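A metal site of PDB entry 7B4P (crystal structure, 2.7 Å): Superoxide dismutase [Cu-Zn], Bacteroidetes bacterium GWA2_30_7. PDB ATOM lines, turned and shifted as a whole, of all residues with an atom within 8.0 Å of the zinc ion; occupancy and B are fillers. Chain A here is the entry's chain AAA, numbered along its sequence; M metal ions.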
ATOM      1  N   PHE A  50     -22.652  16.343 -30.823  1.00  0.00           N
ATOM      2  CA  PHE A  50     -23.266  16.912 -32.049  1.00  0.00           C
ATOM      3  C   PHE A  50     -24.760  17.104 -31.790  1.00  0.00           C
ATOM      4  O   PHE A  50     -25.503  16.094 -31.773  1.00  0.00           O
ATOM      5  CB  PHE A  50     -22.964  15.973 -33.220  1.00  0.00           C
ATOM      6  CG  PHE A  50     -23.287  16.499 -34.602  1.00  0.00           C
ATOM      7  CD1 PHE A  50     -22.596  17.572 -35.142  1.00  0.00           C
ATOM      8  CD2 PHE A  50     -24.249  15.878 -35.383  1.00  0.00           C
ATOM      9  CE1 PHE A  50     -22.886  18.029 -36.413  1.00  0.00           C
ATOM     10  CE2 PHE A  50     -24.541  16.345 -36.657  1.00  0.00           C
ATOM     11  CZ  PHE A  50     -23.863  17.417 -37.167  1.00  0.00           C
ATOM     12  N   HIS A  51     -25.194  18.352 -31.553  1.00  0.00           N
ATOM     13  CA  HIS A  51     -26.565  18.692 -31.073  1.00  0.00           C
ATOM     14  C   HIS A  51     -27.108  19.931 -31.783  1.00  0.00           C
ATOM     15  O   HIS A  51     -26.304  20.762 -32.247  1.00  0.00           O
ATOM     16  CB  HIS A  51     -26.553  18.928 -29.554  1.00  0.00           C
ATOM     17  CG  HIS A  51     -25.877  17.871 -28.753  1.00  0.00           C
ATOM     18  ND1 HIS A  51     -24.827  18.163 -27.898  1.00  0.00           N
ATOM     19  CD2 HIS A  51     -26.087  16.547 -28.658  1.00  0.00           C
ATOM     20  CE1 HIS A  51     -24.419  17.054 -27.319  1.00  0.00           C
ATOM     21  NE2 HIS A  51     -25.182  16.046 -27.763  1.00  0.00           N
ATOM     22  N   ILE A  52     -28.445  20.043 -31.839  1.00  0.00           N
ATOM     23  CA  ILE A  52     -29.183  21.301 -32.155  1.00  0.00           C
ATOM     24  C   ILE A  52     -29.521  21.984 -30.822  1.00  0.00           C
ATOM     25  O   ILE A  52     -30.145  21.328 -29.967  1.00  0.00           O
ATOM     26  CB  ILE A  52     -30.437  21.001 -33.001  1.00  0.00           C
ATOM     27  CG1 ILE A  52     -30.087  20.356 -34.346  1.00  0.00           C
ATOM     28  CG2 ILE A  52     -31.280  22.256 -33.176  1.00  0.00           C
ATOM     29  CD1 ILE A  52     -31.266  19.710 -35.038  1.00  0.00           C
ATOM     30  N   HIS A  53     -29.113  23.245 -30.652  1.00  0.00           N
ATOM     31  CA  HIS A  53     -29.324  24.049 -29.423  1.00  0.00           C
ATOM     32  C   HIS A  53     -30.453  25.066 -29.673  1.00  0.00           C
ATOM     33  O   HIS A  53     -30.674  25.421 -30.845  1.00  0.00           O
ATOM     34  CB  HIS A  53     -28.013  24.699 -28.976  1.00  0.00           C
ATOM     35  CG  HIS A  53     -27.046  23.730 -28.379  1.00  0.00           C
ATOM     36  ND1 HIS A  53     -26.524  23.915 -27.108  1.00  0.00           N
ATOM     37  CD2 HIS A  53     -26.527  22.582 -28.846  1.00  0.00           C
ATOM     38  CE1 HIS A  53     -25.707  22.910 -26.833  1.00  0.00           C
ATOM     39  NE2 HIS A  53     -25.692  22.080 -27.877  1.00  0.00           N
ATOM     40  N   GLY A  68     -29.031  25.989 -24.257  1.00  0.00           N
ATOM     41  CA  GLY A  68     -29.170  24.537 -24.010  1.00  0.00           C
ATOM     42  C   GLY A  68     -29.592  23.790 -25.253  1.00  0.00           C
ATOM     43  O   GLY A  68     -29.819  24.426 -26.298  1.00  0.00           O
ATOM     44  N   HIS A  69     -29.703  22.456 -25.139  1.00  0.00           N
ATOM     45  CA  HIS A  69     -30.171  21.529 -26.207  1.00  0.00           C
ATOM     46  C   HIS A  69     -31.622  21.878 -26.560  1.00  0.00           C
ATOM     47  O   HIS A  69     -32.420  22.048 -25.617  1.00  0.00           O
ATOM     48  CB  HIS A  69     -30.010  20.075 -25.751  1.00  0.00           C
ATOM     49  CG  HIS A  69     -28.592  19.649 -25.573  1.00  0.00           C
ATOM     50  ND1 HIS A  69     -28.222  18.313 -25.546  1.00  0.00           N
ATOM     51  CD2 HIS A  69     -27.450  20.356 -25.419  1.00  0.00           C
ATOM     52  CE1 HIS A  69     -26.913  18.225 -25.378  1.00  0.00           C
ATOM     53  NE2 HIS A  69     -26.421  19.469 -25.307  1.00  0.00           N
ATOM     54  N   PHE A  70     -31.931  21.983 -27.847  1.00  0.00           N
ATOM     55  CA  PHE A  70     -33.297  22.284 -28.363  1.00  0.00           C
ATOM     56  C   PHE A  70     -34.250  21.175 -27.893  1.00  0.00           C
ATOM     57  O   PHE A  70     -34.267  20.089 -28.509  1.00  0.00           O
ATOM     58  CB  PHE A  70     -33.285  22.437 -29.885  1.00  0.00           C
ATOM     59  CG  PHE A  70     -34.631  22.741 -30.498  1.00  0.00           C
ATOM     60  CD1 PHE A  70     -35.419  23.759 -29.998  1.00  0.00           C
ATOM     61  CD2 PHE A  70     -35.095  22.009 -31.582  1.00  0.00           C
ATOM     62  CE1 PHE A  70     -36.657  24.044 -30.553  1.00  0.00           C
ATOM     63  CE2 PHE A  70     -36.333  22.295 -32.137  1.00  0.00           C
ATOM     64  CZ  PHE A  70     -37.113  23.306 -31.628  1.00  0.00           C
ATOM     65  N   ASN A  71     -35.017  21.457 -26.830  1.00  0.00           N
ATOM     66  CA  ASN A  71     -35.860  20.480 -26.090  1.00  0.00           C
ATOM     67  C   ASN A  71     -37.233  21.103 -25.847  1.00  0.00           C
ATOM     68  O   ASN A  71     -37.577  21.423 -24.704  1.00  0.00           O
ATOM     69  CB  ASN A  71     -35.166  20.040 -24.800  1.00  0.00           C
ATOM     70  CG  ASN A  71     -35.928  18.992 -24.031  1.00  0.00           C
ATOM     71  OD1 ASN A  71     -36.777  18.291 -24.586  1.00  0.00           O
ATOM     72  ND2 ASN A  71     -35.631  18.854 -22.749  1.00  0.00           N
ATOM     73  N   LYS A  75     -38.147  16.791 -22.515  1.00  0.00           N
ATOM     74  CA  LYS A  75     -37.743  15.376 -22.344  1.00  0.00           C
ATOM     75  C   LYS A  75     -36.297  15.321 -21.823  1.00  0.00           C
ATOM     76  O   LYS A  75     -35.683  16.390 -21.696  1.00  0.00           O
ATOM     77  CB  LYS A  75     -37.896  14.606 -23.667  1.00  0.00           C
ATOM     78  CG  LYS A  75     -39.303  14.592 -24.247  1.00  0.00           C
ATOM     79  CD  LYS A  75     -39.575  13.434 -25.182  1.00  0.00           C
ATOM     80  CE  LYS A  75     -39.865  12.135 -24.458  1.00  0.00           C
ATOM     81  NZ  LYS A  75     -41.238  12.112 -23.901  1.00  0.00           N
ATOM     82  N   SER A  76     -35.796  14.116 -21.532  1.00  0.00           N
ATOM     83  CA  SER A  76     -34.419  13.859 -21.045  1.00  0.00           C
ATOM     84  C   SER A  76     -33.452  13.802 -22.223  1.00  0.00           C
ATOM     85  O   SER A  76     -33.916  13.649 -23.370  1.00  0.00           O
ATOM     86  CB  SER A  76     -34.362  12.585 -20.231  1.00  0.00           C
ATOM     87  OG  SER A  76     -35.259  12.648 -19.143  1.00  0.00           O
ATOM     88  N   HIS A  77     -32.145  13.934 -21.954  1.00  0.00           N
ATOM     89  CA  HIS A  77     -31.051  13.776 -22.944  1.00  0.00           C
ATOM     90  C   HIS A  77     -30.889  12.296 -23.273  1.00  0.00           C
ATOM     91  O   HIS A  77     -30.952  11.471 -22.348  1.00  0.00           O
ATOM     92  CB  HIS A  77     -29.744  14.378 -22.415  1.00  0.00           C
ATOM     93  CG  HIS A  77     -28.591  14.201 -23.340  1.00  0.00           C
ATOM     94  ND1 HIS A  77     -28.449  14.960 -24.489  1.00  0.00           N
ATOM     95  CD2 HIS A  77     -27.544  13.358 -23.323  1.00  0.00           C
ATOM     96  CE1 HIS A  77     -27.355  14.600 -25.119  1.00  0.00           C
ATOM     97  NE2 HIS A  77     -26.782  13.608 -24.428  1.00  0.00           N
ATOM     98  N   GLY A  78     -30.689  11.966 -24.562  1.00  0.00           N
ATOM     99  CA  GLY A  78     -30.513  10.594 -25.050  1.00  0.00           C
ATOM    100  C   GLY A  78     -29.824  10.542 -26.401  1.00  0.00           C
ATOM    101  O   GLY A  78     -29.249  11.579 -26.805  1.00  0.00           O
ATOM    102  N   ALA A  79     -29.866   9.381 -27.053  1.00  0.00           N
ATOM    103  CA  ALA A  79     -29.287   9.118 -28.390  1.00  0.00           C
ATOM    104  C   ALA A  79     -30.352   9.376 -29.462  1.00  0.00           C
ATOM    105  O   ALA A  79     -31.534   9.433 -29.152  1.00  0.00           O
ATOM    106  CB  ALA A  79     -28.758   7.708 -28.457  1.00  0.00           C
ATOM    107  N   ARG A  85     -35.555  11.441 -25.821  1.00  0.00           N
ATOM    108  CA  ARG A  85     -34.448  12.305 -26.331  1.00  0.00           C
ATOM    109  C   ARG A  85     -34.953  13.739 -26.523  1.00  0.00           C
ATOM    110  O   ARG A  85     -36.181  13.921 -26.675  1.00  0.00           O
ATOM    111  CB  ARG A  85     -33.904  11.753 -27.645  1.00  0.00           C
ATOM    112  CG  ARG A  85     -34.955  11.577 -28.735  1.00  0.00           C
ATOM    113  CD  ARG A  85     -34.371  11.351 -30.122  1.00  0.00           C
ATOM    114  NE  ARG A  85     -33.950  12.587 -30.767  1.00  0.00           N
ATOM    115  CZ  ARG A  85     -33.551  12.693 -32.035  1.00  0.00           C
ATOM    116  NH1 ARG A  85     -33.500  11.622 -32.818  1.00  0.00           N
ATOM    117  NH2 ARG A  85     -33.190  13.872 -32.521  1.00  0.00           N
ATOM    118  N   HIS A  86     -34.031  14.704 -26.547  1.00  0.00           N
ATOM    119  CA  HIS A  86     -34.281  16.099 -27.007  1.00  0.00           C
ATOM    120  C   HIS A  86     -34.417  16.085 -28.537  1.00  0.00           C
ATOM    121  O   HIS A  86     -33.793  15.205 -29.170  1.00  0.00           O
ATOM    122  CB  HIS A  86     -33.169  17.056 -26.553  1.00  0.00           C
ATOM    123  CG  HIS A  86     -32.891  17.046 -25.089  1.00  0.00           C
ATOM    124  ND1 HIS A  86     -31.657  17.400 -24.572  1.00  0.00           N
ATOM    125  CD2 HIS A  86     -33.663  16.708 -24.031  1.00  0.00           C
ATOM    126  CE1 HIS A  86     -31.701  17.295 -23.257  1.00  0.00           C
ATOM    127  NE2 HIS A  86     -32.916  16.871 -22.900  1.00  0.00           N
ATOM    128  N   ILE A  87     -35.184  17.020 -29.108  1.00  0.00           N
ATOM    129  CA  ILE A  87     -35.377  17.168 -30.578  1.00  0.00           C
ATOM    130  C   ILE A  87     -33.997  17.327 -31.237  1.00  0.00           C
ATOM    131  O   ILE A  87     -33.822  16.827 -32.361  1.00  0.00           O
ATOM    132  CB  ILE A  87     -36.317  18.352 -30.894  1.00  0.00           C
ATOM    133  CG1 ILE A  87     -37.750  18.088 -30.426  1.00  0.00           C
ATOM    134  CG2 ILE A  87     -36.272  18.708 -32.377  1.00  0.00           C
ATOM    135  CD1 ILE A  87     -38.487  17.066 -31.250  1.00  0.00           C
ATOM    136  N   GLY A  88     -33.052  17.974 -30.538  1.00  0.00           N
ATOM    137  CA  GLY A  88     -31.690  18.249 -31.026  1.00  0.00           C
ATOM    138  C   GLY A  88     -30.646  17.297 -30.456  1.00  0.00           C
ATOM    139  O   GLY A  88     -29.512  17.753 -30.230  1.00  0.00           O
ATOM    140  N   ASP A  89     -31.005  16.021 -30.250  1.00  0.00           N
ATOM    141  CA  ASP A  89     -30.049  14.941 -29.870  1.00  0.00           C
ATOM    142  C   ASP A  89     -29.664  14.168 -31.130  1.00  0.00           C
ATOM    143  O   ASP A  89     -30.318  13.148 -31.429  1.00  0.00           O
ATOM    144  CB  ASP A  89     -30.630  14.023 -28.785  1.00  0.00           C
ATOM    145  CG  ASP A  89     -30.572  14.593 -27.378  1.00  0.00           C
ATOM    146  OD1 ASP A  89     -29.964  15.667 -27.200  1.00  0.00           O
ATOM    147  OD2 ASP A  89     -31.126  13.957 -26.470  1.00  0.00           O
ATOM    148  N   LEU A  90     -28.632  14.640 -31.837  1.00  0.00           N
ATOM    149  CA  LEU A  90     -28.098  14.015 -33.083  1.00  0.00           C
ATOM    150  C   LEU A  90     -26.863  13.161 -32.736  1.00  0.00           C
ATOM    151  O   LEU A  90     -26.092  12.835 -33.667  1.00  0.00           O
ATOM    152  CB  LEU A  90     -27.752  15.108 -34.106  1.00  0.00           C
ATOM    153  CG  LEU A  90     -28.779  16.237 -34.249  1.00  0.00           C
ATOM    154  CD1 LEU A  90     -28.405  17.154 -35.402  1.00  0.00           C
ATOM    155  CD2 LEU A  90     -30.192  15.701 -34.451  1.00  0.00           C
ATOM    156  N   GLY A  91     -26.691  12.815 -31.456  1.00  0.00           N
ATOM    157  CA  GLY A  91     -25.649  11.904 -30.958  1.00  0.00           C
ATOM    158  C   GLY A  91     -24.249  12.491 -31.091  1.00  0.00           C
ATOM    159  O   GLY A  91     -24.054  13.650 -30.675  1.00  0.00           O
ATOM    160  N   HIS A 126     -19.109  19.685 -29.793  1.00  0.00           N
ATOM    161  CA  HIS A 126     -18.473  19.700 -28.446  1.00  0.00           C
ATOM    162  C   HIS A 126     -17.046  19.168 -28.540  1.00  0.00           C
ATOM    163  O   HIS A 126     -16.739  18.483 -29.539  1.00  0.00           O
ATOM    164  CB  HIS A 126     -19.323  18.920 -27.443  1.00  0.00           C
ATOM    165  CG  HIS A 126     -20.640  19.563 -27.146  1.00  0.00           C
ATOM    166  ND1 HIS A 126     -20.814  20.447 -26.105  1.00  0.00           N
ATOM    167  CD2 HIS A 126     -21.838  19.473 -27.769  1.00  0.00           C
ATOM    168  CE1 HIS A 126     -22.073  20.860 -26.085  1.00  0.00           C
ATOM    169  NE2 HIS A 126     -22.713  20.277 -27.098  1.00  0.00           N
ATOM    170  N   ASP A 130     -20.250  12.803 -26.383  1.00  0.00           N
ATOM    171  CA  ASP A 130     -21.591  12.726 -25.735  1.00  0.00           C
ATOM    172  C   ASP A 130     -21.841  11.255 -25.364  1.00  0.00           C
ATOM    173  O   ASP A 130     -22.016  10.442 -26.289  1.00  0.00           O
ATOM    174  CB  ASP A 130     -22.670  13.295 -26.652  1.00  0.00           C
ATOM    175  CG  ASP A 130     -24.093  13.111 -26.164  1.00  0.00           C
ATOM    176  OD1 ASP A 130     -24.269  12.617 -25.032  1.00  0.00           O
ATOM    177  OD2 ASP A 130     -25.024  13.456 -26.914  1.00  0.00           O
ATOM    178  N   THR A 134     -25.434  10.773 -19.272  1.00  0.00           N
ATOM    179  CA  THR A 134     -25.323  11.910 -18.309  1.00  0.00           C
ATOM    180  C   THR A 134     -26.309  13.007 -18.695  1.00  0.00           C
ATOM    181  O   THR A 134     -26.531  13.224 -19.905  1.00  0.00           O
ATOM    182  CB  THR A 134     -23.883  12.438 -18.238  1.00  0.00           C
ATOM    183  OG1 THR A 134     -23.005  11.330 -18.035  1.00  0.00           O
ATOM    184  CG2 THR A 134     -23.673  13.445 -17.137  1.00  0.00           C
ATOM    185  N   GLN A 135     -26.891  13.681 -17.686  1.00  0.00           N
ATOM    186  CA  GLN A 135     -27.935  14.727 -17.856  1.00  0.00           C
ATOM    187  C   GLN A 135     -27.374  16.080 -17.417  1.00  0.00           C
ATOM    188  O   GLN A 135     -26.595  16.147 -16.464  1.00  0.00           O
ATOM    189  CB  GLN A 135     -29.176  14.361 -17.043  1.00  0.00           C
ATOM    190  CG  GLN A 135     -29.824  13.050 -17.465  1.00  0.00           C
ATOM    191  CD  GLN A 135     -30.430  13.121 -18.846  1.00  0.00           C
ATOM    192  OE1 GLN A 135     -30.931  14.154 -19.283  1.00  0.00           O
ATOM    193  NE2 GLN A 135     -30.403  11.998 -19.554  1.00  0.00           N
ATOM    194  N   PRO A 136     -27.741  17.208 -18.076  1.00  0.00           N
ATOM    195  CA  PRO A 136     -28.588  17.200 -19.263  1.00  0.00           C
ATOM    196  C   PRO A 136     -27.825  17.229 -20.603  1.00  0.00           C
ATOM    197  O   PRO A 136     -28.473  17.365 -21.634  1.00  0.00           O
ATOM    198  CB  PRO A 136     -29.338  18.523 -19.066  1.00  0.00           C
ATOM    199  CG  PRO A 136     -28.281  19.459 -18.502  1.00  0.00           C
ATOM    200  CD  PRO A 136     -27.379  18.571 -17.671  1.00  0.00           C
ATOM    201  N   THR A 137     -26.495  17.101 -20.564  1.00  0.00           N
ATOM    202  CA  THR A 137     -25.566  17.417 -21.688  1.00  0.00           C
ATOM    203  C   THR A 137     -24.965  16.138 -22.285  1.00  0.00           C
ATOM    204  O   THR A 137     -24.618  16.168 -23.486  1.00  0.00           O
ATOM    205  CB  THR A 137     -24.453  18.349 -21.212  1.00  0.00           C
ATOM    206  OG1 THR A 137     -23.832  17.761 -20.076  1.00  0.00           O
ATOM    207  CG2 THR A 137     -24.970  19.727 -20.846  1.00  0.00           C
ATOM    208  N   GLY A 138     -24.826  15.070 -21.498  1.00  0.00           N
ATOM    209  CA  GLY A 138     -24.076  13.850 -21.868  1.00  0.00           C
ATOM    210  C   GLY A 138     -22.580  14.008 -21.614  1.00  0.00           C
ATOM    211  O   GLY A 138     -21.804  13.223 -22.172  1.00  0.00           O
HETATM  212 ZN    ZN M   1     -29.636  16.866 -25.440  1.00  0.00          ZN
HETATM  213 CU    CU M   2     -24.729  20.293 -27.513  1.00  0.00          CU
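A ring nitrogen (NE2) of His 69 sits close to a ring nitrogen (ND1) of His 51 (3.3 Å).
The backbone NH (N) of Gly 78 is in hydrogen-bond range of the side-chain carboxylate (OD2) of Asp 89 (2.8 Å).
The backbone carbonyl oxygen (O) of Asp 89 is in hydrogen-bond range of the guanidinium group (NH2) of Arg 85 (3.2 Å).
The backbone NH (N) of His 86 lies close to the backbone carbonyl oxygen (O) of Ser 76.
A ring nitrogen (NE2) of His 86 lies close to the side-chain amide nitrogen (ND2) of Asn 71 (3.4 Å).
NE2 of His 86 is in hydrogen-bond range of O of Lys 75, at 3.1 Å.
The side-chain carboxylate of Asp 130 lies within hydrogen-bond range of a ring nitrogen (NE2) of His 77, at 2.8 Å.
The backbone carbonyl oxygen (O) of His 77 sits at hydrogen-bond distance from the side-chain amide nitrogen (NE2) of Gln 135 (2.9 Å).
Of the 27 residues printed, 4 come within 4 Å of the zinc ion.
The nearest printed residue that does not touch the zinc ion is Pro 136 (4.01 Å).
The zinc ion is bound by ND1 of His 69 (2.0 Å), OD1 of Asp 89 (2.2 Å), ND1 of His 86 (2.3 Å) and ND1 of His 77 (2.4 Å).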
